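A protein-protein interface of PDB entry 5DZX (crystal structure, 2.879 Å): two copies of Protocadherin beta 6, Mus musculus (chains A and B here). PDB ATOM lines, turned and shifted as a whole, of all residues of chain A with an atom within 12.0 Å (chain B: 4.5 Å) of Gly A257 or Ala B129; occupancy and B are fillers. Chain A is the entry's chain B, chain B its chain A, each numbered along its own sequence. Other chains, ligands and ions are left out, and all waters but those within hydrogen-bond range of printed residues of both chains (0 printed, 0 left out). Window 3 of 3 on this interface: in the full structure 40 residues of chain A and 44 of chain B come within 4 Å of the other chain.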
ATOM      1  N   LEU A 253       7.648  16.138  -9.932  1.00  0.00           N
ATOM      2  CA  LEU A 253       6.254  15.967 -10.326  1.00  0.00           C
ATOM      3  C   LEU A 253       6.091  15.314 -11.690  1.00  0.00           C
ATOM      4  O   LEU A 253       6.914  15.494 -12.588  1.00  0.00           O
ATOM      5  CB  LEU A 253       5.519  17.319 -10.313  1.00  0.00           C
ATOM      6  CG  LEU A 253       5.885  18.478 -11.257  1.00  0.00           C
ATOM      7  CD1 LEU A 253       5.378  18.296 -12.684  1.00  0.00           C
ATOM      8  CD2 LEU A 253       5.349  19.787 -10.695  1.00  0.00           C
ATOM      9  N   PHE A 254       5.000  14.571 -11.832  1.00  0.00           N
ATOM     10  CA  PHE A 254       4.608  13.988 -13.104  1.00  0.00           C
ATOM     11  C   PHE A 254       3.231  14.516 -13.472  1.00  0.00           C
ATOM     12  O   PHE A 254       2.220  14.104 -12.898  1.00  0.00           O
ATOM     13  CB  PHE A 254       4.598  12.457 -13.042  1.00  0.00           C
ATOM     14  CG  PHE A 254       5.947  11.842 -12.776  1.00  0.00           C
ATOM     15  CD1 PHE A 254       7.107  12.472 -13.192  1.00  0.00           C
ATOM     16  CD2 PHE A 254       6.052  10.629 -12.116  1.00  0.00           C
ATOM     17  CE1 PHE A 254       8.347  11.907 -12.950  1.00  0.00           C
ATOM     18  CE2 PHE A 254       7.287  10.060 -11.872  1.00  0.00           C
ATOM     19  CZ  PHE A 254       8.436  10.700 -12.290  1.00  0.00           C
ATOM     20  N   GLN A 255       3.203  15.438 -14.426  1.00  0.00           N
ATOM     21  CA  GLN A 255       1.949  15.970 -14.931  1.00  0.00           C
ATOM     22  C   GLN A 255       1.272  14.934 -15.813  1.00  0.00           C
ATOM     23  O   GLN A 255       1.892  13.948 -16.209  1.00  0.00           O
ATOM     24  CB  GLN A 255       2.188  17.268 -15.700  1.00  0.00           C
ATOM     25  CG  GLN A 255       3.228  17.158 -16.800  1.00  0.00           C
ATOM     26  CD  GLN A 255       3.469  18.480 -17.498  1.00  0.00           C
ATOM     27  OE1 GLN A 255       2.892  19.503 -17.129  1.00  0.00           O
ATOM     28  NE2 GLN A 255       4.323  18.467 -18.514  1.00  0.00           N
ATOM     29  N   GLY A 256      -0.002  15.158 -16.117  1.00  0.00           N
ATOM     30  CA  GLY A 256      -0.751  14.248 -16.962  1.00  0.00           C
ATOM     31  C   GLY A 256      -0.123  14.100 -18.334  1.00  0.00           C
ATOM     32  O   GLY A 256       0.603  14.981 -18.797  1.00  0.00           O
ATOM     33  N   GLY A 257      -0.393  12.967 -18.975  1.00  0.00           N
ATOM     34  CA  GLY A 257       0.117  12.695 -20.303  1.00  0.00           C
ATOM     35  C   GLY A 257      -0.336  13.735 -21.308  1.00  0.00           C
ATOM     36  O   GLY A 257       0.443  14.176 -22.150  1.00  0.00           O
ATOM     37  N   GLY A 258      -1.601  14.127 -21.215  1.00  0.00           N
ATOM     38  CA  GLY A 258      -2.156  15.114 -22.119  1.00  0.00           C
ATOM     39  C   GLY A 258      -2.145  16.525 -21.567  1.00  0.00           C
ATOM     40  O   GLY A 258      -2.566  16.768 -20.435  1.00  0.00           O
ATOM     41  N   GLY A 259      -1.645  17.458 -22.371  1.00  0.00           N
ATOM     42  CA  GLY A 259      -1.698  18.867 -22.030  1.00  0.00           C
ATOM     43  C   GLY A 259      -0.672  19.298 -21.002  1.00  0.00           C
ATOM     44  O   GLY A 259      -0.559  18.691 -19.936  1.00  0.00           O
ATOM     45  N   PRO A 260       0.077  20.366 -21.312  1.00  0.00           N
ATOM     46  CA  PRO A 260       1.044  20.928 -20.367  1.00  0.00           C
ATOM     47  C   PRO A 260       0.335  21.571 -19.183  1.00  0.00           C
ATOM     48  O   PRO A 260      -0.809  22.004 -19.315  1.00  0.00           O
ATOM     49  CB  PRO A 260       1.785  21.971 -21.206  1.00  0.00           C
ATOM     50  CG  PRO A 260       0.786  22.387 -22.229  1.00  0.00           C
ATOM     51  CD  PRO A 260       0.042  21.125 -22.573  1.00  0.00           C
ATOM     52  N   GLN A 261       1.004  21.622 -18.038  1.00  0.00           N
ATOM     53  CA  GLN A 261       0.403  22.188 -16.839  1.00  0.00           C
ATOM     54  C   GLN A 261       1.236  23.350 -16.314  1.00  0.00           C
ATOM     55  O   GLN A 261       2.457  23.354 -16.458  1.00  0.00           O
ATOM     56  CB  GLN A 261       0.254  21.110 -15.766  1.00  0.00           C
ATOM     57  CG  GLN A 261      -0.665  19.969 -16.170  1.00  0.00           C
ATOM     58  CD  GLN A 261      -0.853  18.956 -15.058  1.00  0.00           C
ATOM     59  OE1 GLN A 261      -0.140  18.981 -14.056  1.00  0.00           O
ATOM     60  NE2 GLN A 261      -1.812  18.054 -15.234  1.00  0.00           N
ATOM     61  N   PRO A 262       0.574  24.343 -15.703  1.00  0.00           N
ATOM     62  CA  PRO A 262       1.276  25.492 -15.128  1.00  0.00           C
ATOM     63  C   PRO A 262       1.716  25.248 -13.687  1.00  0.00           C
ATOM     64  O   PRO A 262       1.767  26.186 -12.894  1.00  0.00           O
ATOM     65  CB  PRO A 262       0.232  26.617 -15.199  1.00  0.00           C
ATOM     66  CG  PRO A 262      -1.091  25.945 -15.565  1.00  0.00           C
ATOM     67  CD  PRO A 262      -0.882  24.463 -15.534  1.00  0.00           C
ATOM     68  N   PHE A 263       2.020  23.999 -13.353  1.00  0.00           N
ATOM     69  CA  PHE A 263       2.475  23.658 -12.009  1.00  0.00           C
ATOM     70  C   PHE A 263       3.958  23.302 -11.980  1.00  0.00           C
ATOM     71  O   PHE A 263       4.464  22.627 -12.877  1.00  0.00           O
ATOM     72  CB  PHE A 263       1.646  22.501 -11.448  1.00  0.00           C
ATOM     73  CG  PHE A 263       0.201  22.844 -11.238  1.00  0.00           C
ATOM     74  CD1 PHE A 263      -0.161  24.086 -10.745  1.00  0.00           C
ATOM     75  CD2 PHE A 263      -0.793  21.930 -11.541  1.00  0.00           C
ATOM     76  CE1 PHE A 263      -1.489  24.407 -10.550  1.00  0.00           C
ATOM     77  CE2 PHE A 263      -2.125  22.248 -11.350  1.00  0.00           C
ATOM     78  CZ  PHE A 263      -2.472  23.488 -10.853  1.00  0.00           C
ATOM     79  N   THR A 283      -9.474  24.832 -18.708  1.00  0.00           N
ATOM     80  CA  THR A 283      -9.251  23.581 -17.989  1.00  0.00           C
ATOM     81  C   THR A 283      -9.981  23.581 -16.648  1.00  0.00           C
ATOM     82  O   THR A 283      -9.710  24.418 -15.788  1.00  0.00           O
ATOM     83  CB  THR A 283      -7.752  23.338 -17.751  1.00  0.00           C
ATOM     84  OG1 THR A 283      -7.188  24.462 -17.063  1.00  0.00           O
ATOM     85  CG2 THR A 283      -7.028  23.148 -19.079  1.00  0.00           C
ATOM     86  N   TYR A 285     -10.158  20.913 -14.452  1.00  0.00           N
ATOM     87  CA  TYR A 285      -9.533  20.076 -13.441  1.00  0.00           C
ATOM     88  C   TYR A 285      -8.134  19.649 -13.862  1.00  0.00           C
ATOM     89  O   TYR A 285      -7.854  19.469 -15.047  1.00  0.00           O
ATOM     90  CB  TYR A 285     -10.399  18.849 -13.150  1.00  0.00           C
ATOM     91  CG  TYR A 285     -10.172  17.693 -14.095  1.00  0.00           C
ATOM     92  CD1 TYR A 285     -10.714  17.694 -15.374  1.00  0.00           C
ATOM     93  CD2 TYR A 285      -9.419  16.593 -13.702  1.00  0.00           C
ATOM     94  CE1 TYR A 285     -10.507  16.635 -16.238  1.00  0.00           C
ATOM     95  CE2 TYR A 285      -9.208  15.530 -14.557  1.00  0.00           C
ATOM     96  CZ  TYR A 285      -9.753  15.554 -15.823  1.00  0.00           C
ATOM     97  OH  TYR A 285      -9.541  14.493 -16.674  1.00  0.00           O
ATOM     98  N   TYR A 286      -7.254  19.500 -12.879  1.00  0.00           N
ATOM     99  CA  TYR A 286      -5.899  19.031 -13.124  1.00  0.00           C
ATOM    100  C   TYR A 286      -5.592  17.819 -12.256  1.00  0.00           C
ATOM    101  O   TYR A 286      -5.879  17.812 -11.064  1.00  0.00           O
ATOM    102  CB  TYR A 286      -4.890  20.145 -12.855  1.00  0.00           C
ATOM    103  CG  TYR A 286      -4.802  21.166 -13.960  1.00  0.00           C
ATOM    104  CD1 TYR A 286      -4.715  20.772 -15.286  1.00  0.00           C
ATOM    105  CD2 TYR A 286      -4.809  22.526 -13.677  1.00  0.00           C
ATOM    106  CE1 TYR A 286      -4.631  21.703 -16.302  1.00  0.00           C
ATOM    107  CE2 TYR A 286      -4.726  23.465 -14.686  1.00  0.00           C
ATOM    108  CZ  TYR A 286      -4.636  23.049 -15.997  1.00  0.00           C
ATOM    109  OH  TYR A 286      -4.552  23.979 -17.006  1.00  0.00           O
ATOM    110  N   THR A 287      -5.007  16.790 -12.853  1.00  0.00           N
ATOM    111  CA  THR A 287      -4.637  15.603 -12.098  1.00  0.00           C
ATOM    112  C   THR A 287      -3.197  15.209 -12.416  1.00  0.00           C
ATOM    113  O   THR A 287      -2.801  15.134 -13.583  1.00  0.00           O
ATOM    114  CB  THR A 287      -5.598  14.426 -12.382  1.00  0.00           C
ATOM    115  OG1 THR A 287      -5.043  13.213 -11.864  1.00  0.00           O
ATOM    116  CG2 THR A 287      -5.849  14.275 -13.878  1.00  0.00           C
ATOM    117  N   MET A 288      -2.413  14.983 -11.367  1.00  0.00           N
ATOM    118  CA  MET A 288      -1.000  14.662 -11.526  1.00  0.00           C
ATOM    119  C   MET A 288      -0.513  13.754 -10.412  1.00  0.00           C
ATOM    120  O   MET A 288      -1.238  13.493  -9.457  1.00  0.00           O
ATOM    121  CB  MET A 288      -0.170  15.942 -11.556  1.00  0.00           C
ATOM    122  CG  MET A 288      -0.389  16.832 -10.348  1.00  0.00           C
ATOM    123  SD  MET A 288       0.125  18.526 -10.671  1.00  0.00           S
ATOM    124  CE  MET A 288      -0.280  19.304  -9.111  1.00  0.00           C
ATOM    125  N   GLU A 289       0.715  13.265 -10.538  1.00  0.00           N
ATOM    126  CA  GLU A 289       1.287  12.389  -9.522  1.00  0.00           C
ATOM    127  C   GLU A 289       2.635  12.901  -9.042  1.00  0.00           C
ATOM    128  O   GLU A 289       3.539  13.109  -9.840  1.00  0.00           O
ATOM    129  CB  GLU A 289       1.429  10.966 -10.061  1.00  0.00           C
ATOM    130  CG  GLU A 289       0.105  10.276 -10.338  1.00  0.00           C
ATOM    131  CD  GLU A 289       0.279   8.925 -11.001  1.00  0.00           C
ATOM    132  OE1 GLU A 289       1.423   8.587 -11.364  1.00  0.00           O
ATOM    133  OE2 GLU A 289      -0.728   8.204 -11.164  1.00  0.00           O
ATOM    134  N   ILE A 290       2.758  13.122  -7.738  1.00  0.00           N
ATOM    135  CA  ILE A 290       4.022  13.566  -7.157  1.00  0.00           C
ATOM    136  C   ILE A 290       4.864  12.376  -6.707  1.00  0.00           C
ATOM    137  O   ILE A 290       4.390  11.524  -5.953  1.00  0.00           O
ATOM    138  CB  ILE A 290       3.791  14.501  -5.960  1.00  0.00           C
ATOM    139  CG1 ILE A 290       2.989  15.722  -6.398  1.00  0.00           C
ATOM    140  CG2 ILE A 290       5.112  14.928  -5.348  1.00  0.00           C
ATOM    141  CD1 ILE A 290       3.746  16.643  -7.316  1.00  0.00           C
ATOM    142  N   LYS A 301       5.148   7.213  -4.322  1.00  0.00           N
ATOM    143  CA  LYS A 301       4.333   8.069  -5.175  1.00  0.00           C
ATOM    144  C   LYS A 301       2.981   8.406  -4.551  1.00  0.00           C
ATOM    145  O   LYS A 301       2.363   7.574  -3.886  1.00  0.00           O
ATOM    146  CB  LYS A 301       4.132   7.406  -6.539  1.00  0.00           C
ATOM    147  CG  LYS A 301       3.388   8.265  -7.547  1.00  0.00           C
ATOM    148  CD  LYS A 301       3.163   7.521  -8.849  1.00  0.00           C
ATOM    149  CE  LYS A 301       2.230   6.336  -8.667  1.00  0.00           C
ATOM    150  NZ  LYS A 301       2.008   5.611  -9.950  1.00  0.00           N
ATOM    151  N   THR A 303      -0.828  10.936  -5.329  1.00  0.00           N
ATOM    152  CA  THR A 303      -1.646  11.591  -6.347  1.00  0.00           C
ATOM    153  C   THR A 303      -2.144  12.950  -5.867  1.00  0.00           C
ATOM    154  O   THR A 303      -2.632  13.083  -4.746  1.00  0.00           O
ATOM    155  CB  THR A 303      -2.856  10.725  -6.744  1.00  0.00           C
ATOM    156  OG1 THR A 303      -2.399   9.459  -7.238  1.00  0.00           O
ATOM    157  CG2 THR A 303      -3.677  11.413  -7.826  1.00  0.00           C
ATOM    158  N   VAL A 304      -2.012  13.956  -6.725  1.00  0.00           N
ATOM    159  CA  VAL A 304      -2.491  15.297  -6.420  1.00  0.00           C
ATOM    160  C   VAL A 304      -3.518  15.759  -7.450  1.00  0.00           C
ATOM    161  O   VAL A 304      -3.280  15.695  -8.662  1.00  0.00           O
ATOM    162  CB  VAL A 304      -1.336  16.311  -6.360  1.00  0.00           C
ATOM    163  CG1 VAL A 304      -1.878  17.725  -6.208  1.00  0.00           C
ATOM    164  CG2 VAL A 304      -0.403  15.972  -5.209  1.00  0.00           C
ATOM    165  N   GLU B 104       5.722  15.043 -27.803  1.00  0.00           N
ATOM    166  CA  GLU B 104       6.867  15.810 -27.338  1.00  0.00           C
ATOM    167  C   GLU B 104       7.096  15.607 -25.844  1.00  0.00           C
ATOM    168  O   GLU B 104       6.145  15.488 -25.074  1.00  0.00           O
ATOM    169  CB  GLU B 104       6.663  17.296 -27.645  1.00  0.00           C
ATOM    170  CG  GLU B 104       7.862  18.168 -27.326  1.00  0.00           C
ATOM    171  CD  GLU B 104       7.595  19.637 -27.574  1.00  0.00           C
ATOM    172  OE1 GLU B 104       6.515  19.965 -28.112  1.00  0.00           O
ATOM    173  OE2 GLU B 104       8.462  20.463 -27.223  1.00  0.00           O
ATOM    174  N   PHE B 105       8.365  15.570 -25.444  1.00  0.00           N
ATOM    175  CA  PHE B 105       8.728  15.395 -24.042  1.00  0.00           C
ATOM    176  C   PHE B 105       9.069  16.719 -23.373  1.00  0.00           C
ATOM    177  O   PHE B 105       9.803  17.534 -23.935  1.00  0.00           O
ATOM    178  CB  PHE B 105       9.903  14.431 -23.905  1.00  0.00           C
ATOM    179  CG  PHE B 105       9.516  12.988 -24.014  1.00  0.00           C
ATOM    180  CD1 PHE B 105       9.036  12.306 -22.909  1.00  0.00           C
ATOM    181  CD2 PHE B 105       9.629  12.313 -25.215  1.00  0.00           C
ATOM    182  CE1 PHE B 105       8.678  10.976 -23.000  1.00  0.00           C
ATOM    183  CE2 PHE B 105       9.271  10.982 -25.312  1.00  0.00           C
ATOM    184  CZ  PHE B 105       8.795  10.313 -24.203  1.00  0.00           C
ATOM    185  N   LYS B 127       8.551  10.345 -16.850  1.00  0.00           N
ATOM    186  CA  LYS B 127       7.680  11.406 -17.331  1.00  0.00           C
ATOM    187  C   LYS B 127       7.074  11.020 -18.676  1.00  0.00           C
ATOM    188  O   LYS B 127       7.671  10.264 -19.440  1.00  0.00           O
ATOM    189  CB  LYS B 127       8.450  12.722 -17.429  1.00  0.00           C
ATOM    190  CG  LYS B 127       9.044  13.157 -16.099  1.00  0.00           C
ATOM    191  CD  LYS B 127       9.903  14.398 -16.225  1.00  0.00           C
ATOM    192  CE  LYS B 127      10.391  14.851 -14.859  1.00  0.00           C
ATOM    193  NZ  LYS B 127      11.270  16.047 -14.940  1.00  0.00           N
ATOM    194  N   ALA B 128       5.877  11.525 -18.951  1.00  0.00           N
ATOM    195  CA  ALA B 128       5.151  11.141 -20.155  1.00  0.00           C
ATOM    196  C   ALA B 128       5.242  12.220 -21.226  1.00  0.00           C
ATOM    197  O   ALA B 128       5.434  13.398 -20.922  1.00  0.00           O
ATOM    198  CB  ALA B 128       3.698  10.847 -19.823  1.00  0.00           C
ATOM    199  N   ALA B 129       5.107  11.809 -22.483  1.00  0.00           N
ATOM    200  CA  ALA B 129       5.143  12.740 -23.601  1.00  0.00           C
ATOM    201  C   ALA B 129       3.795  13.424 -23.775  1.00  0.00           C
ATOM    202  O   ALA B 129       2.757  12.765 -23.836  1.00  0.00           O
ATOM    203  CB  ALA B 129       5.543  12.022 -24.880  1.00  0.00           C
ATOM    204  N   GLN B 130       3.815  14.751 -23.842  1.00  0.00           N
ATOM    205  CA  GLN B 130       2.586  15.522 -23.978  1.00  0.00           C
ATOM    206  C   GLN B 130       2.124  15.594 -25.431  1.00  0.00           C
ATOM    207  O   GLN B 130       2.912  15.862 -26.339  1.00  0.00           O
ATOM    208  CB  GLN B 130       2.770  16.927 -23.400  1.00  0.00           C
ATOM    209  CG  GLN B 130       4.071  17.604 -23.793  1.00  0.00           C
ATOM    210  CD  GLN B 130       4.438  18.735 -22.853  1.00  0.00           C
ATOM    211  OE1 GLN B 130       3.794  18.935 -21.822  1.00  0.00           O
ATOM    212  NE2 GLN B 130       5.479  19.482 -23.202  1.00  0.00           N
ATOM    213  N   ASP B 131       0.834  15.351 -25.635  1.00  0.00           N
ATOM    214  CA  ASP B 131       0.231  15.414 -26.959  1.00  0.00           C
ATOM    215  C   ASP B 131      -1.113  16.126 -26.882  1.00  0.00           C
ATOM    216  O   ASP B 131      -1.942  15.805 -26.031  1.00  0.00           O
ATOM    217  CB  ASP B 131       0.062  14.010 -27.542  1.00  0.00           C
ATOM    218  CG  ASP B 131      -0.118  14.020 -29.051  1.00  0.00           C
ATOM    219  OD1 ASP B 131      -0.723  14.978 -29.577  1.00  0.00           O
ATOM    220  OD2 ASP B 131       0.347  13.069 -29.714  1.00  0.00           O
ATOM    221  N   VAL B 139      -0.556   9.788 -28.109  1.00  0.00           N
ATOM    222  CA  VAL B 139       0.508   8.825 -27.862  1.00  0.00           C
ATOM    223  C   VAL B 139      -0.102   7.444 -27.631  1.00  0.00           C
ATOM    224  O   VAL B 139      -1.058   7.304 -26.869  1.00  0.00           O
ATOM    225  CB  VAL B 139       1.368   9.240 -26.659  1.00  0.00           C
ATOM    226  CG1 VAL B 139       2.430   8.194 -26.386  1.00  0.00           C
ATOM    227  CG2 VAL B 139       2.015  10.588 -26.922  1.00  0.00           C
ATOM    228  N   TYR B 142       5.151   3.135 -26.423  1.00  0.00           N
ATOM    229  CA  TYR B 142       6.420   3.606 -25.870  1.00  0.00           C
ATOM    230  C   TYR B 142       7.530   2.593 -26.112  1.00  0.00           C
ATOM    231  O   TYR B 142       7.384   1.414 -25.787  1.00  0.00           O
ATOM    232  CB  TYR B 142       6.296   3.889 -24.371  1.00  0.00           C
ATOM    233  CG  TYR B 142       5.794   5.277 -24.038  1.00  0.00           C
ATOM    234  CD1 TYR B 142       6.634   6.381 -24.125  1.00  0.00           C
ATOM    235  CD2 TYR B 142       4.485   5.481 -23.623  1.00  0.00           C
ATOM    236  CE1 TYR B 142       6.179   7.651 -23.817  1.00  0.00           C
ATOM    237  CE2 TYR B 142       4.022   6.747 -23.311  1.00  0.00           C
ATOM    238  CZ  TYR B 142       4.873   7.828 -23.411  1.00  0.00           C
ATOM    239  OH  TYR B 142       4.409   9.088 -23.100  1.00  0.00           O
ATOM    240  N   ARG B 161      -5.409   8.666 -21.712  1.00  0.00           N
ATOM    241  CA  ARG B 161      -4.139   8.273 -22.321  1.00  0.00           C
ATOM    242  C   ARG B 161      -3.324   7.308 -21.461  1.00  0.00           C
ATOM    243  O   ARG B 161      -3.828   6.735 -20.493  1.00  0.00           O
ATOM    244  CB  ARG B 161      -3.303   9.515 -22.638  1.00  0.00           C
ATOM    245  CG  ARG B 161      -4.031  10.540 -23.486  1.00  0.00           C
ATOM    246  CD  ARG B 161      -3.243  11.832 -23.591  1.00  0.00           C
ATOM    247  NE  ARG B 161      -4.021  12.883 -24.236  1.00  0.00           N
ATOM    248  CZ  ARG B 161      -4.884  13.667 -23.597  1.00  0.00           C
ATOM    249  NH1 ARG B 161      -5.079  13.517 -22.292  1.00  0.00           N
ATOM    250  NH2 ARG B 161      -5.552  14.601 -24.261  1.00  0.00           N
ATOM    251  N   ALA B 186       8.472   8.055 -28.013  1.00  0.00           N
ATOM    252  CA  ALA B 186       7.021   7.988 -27.916  1.00  0.00           C
ATOM    253  C   ALA B 186       6.394   7.890 -29.304  1.00  0.00           C
ATOM    254  O   ALA B 186       6.539   8.790 -30.133  1.00  0.00           O
ATOM    255  CB  ALA B 186       6.485   9.196 -27.175  1.00  0.00           C
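O of Glu B104 is in hydrogen-bond range of N of Gln B130 (2.7 Å).
N of Ala B129 is in hydrogen-bond range of OH of Tyr B142 (2.9 Å).
N of Phe A254 sits at hydrogen-bond distance from O of Glu A289 (2.9 Å).
The backbone NH (N) of Gln A261 sits at hydrogen-bond distance from the side-chain amide oxygen (OE1) of Gln A255, 3.0 Å away.
Among the printed residues, merely in contact across the chains: Phe A254 with Lys B127, Gly A257 with Gln B130, Gly A257 with Asp B131, Gly A258 with Asp B131, Gly A258 with Arg B161 and Pro A260 with Gln B130.
Hydrophobic or aromatic side chains of chain A that line the printed part of chain B: Phe A254 and Pro A260.
Of the 11 printed residues of chain B, 5 touch a printed residue of chain A.
Printed residues of chain B that touch a printed residue of chain A: Lys B127, Ala B129, Gln B130, Asp B131 and Arg B161.
Among the printed residues, 8 pairs touch across the chains.
The side-chain amide oxygen (OE1) of Gln B130 is in hydrogen-bond range of the side-chain amide nitrogen (NE2) of Gln A255 (3.4 Å).
The backbone carbonyl oxygen (O) of Gly A257 sits close to the backbone carbonyl oxygen (O) of Ala B129 (3.2 Å).
Of the printed residues of chain B, Phe A254 touches Lys B127.
Of the printed residues of chain B, Gln A255 touches Gln B130.
Of chain B, only Ala B129, Gln B130 and Asp B131 come within 4 Å of Gly A257.
Printed residues of chain B within 4 Å of Gly A258: Asp B131 (3.98 Å) and Arg B161 (3.3 Å).
Printed residues of chain B within 4 Å of Pro A260: Gln B130.
Gln A261 touches none of the printed residues of chain B.
Of the printed residues of chain A, Lys B127 touches Phe A254.
No residue of chain A comes within 4 Å of Ala B128.
Of chain A, only Gly A257 comes within 4 Å of Ala B129.
Gln B130 touches just these residues of chain A: Gln A255, Gly A257 and Pro A260.
Of the printed residues of chain A, Asp B131 touches Gly A257 and Gly A258.
No residue of chain A comes within 4 Å of Val B139.
The nearest residue of chain B that does not touch Gly A257 is Ala B128 (4.1 Å).
No position is printed for both chains.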
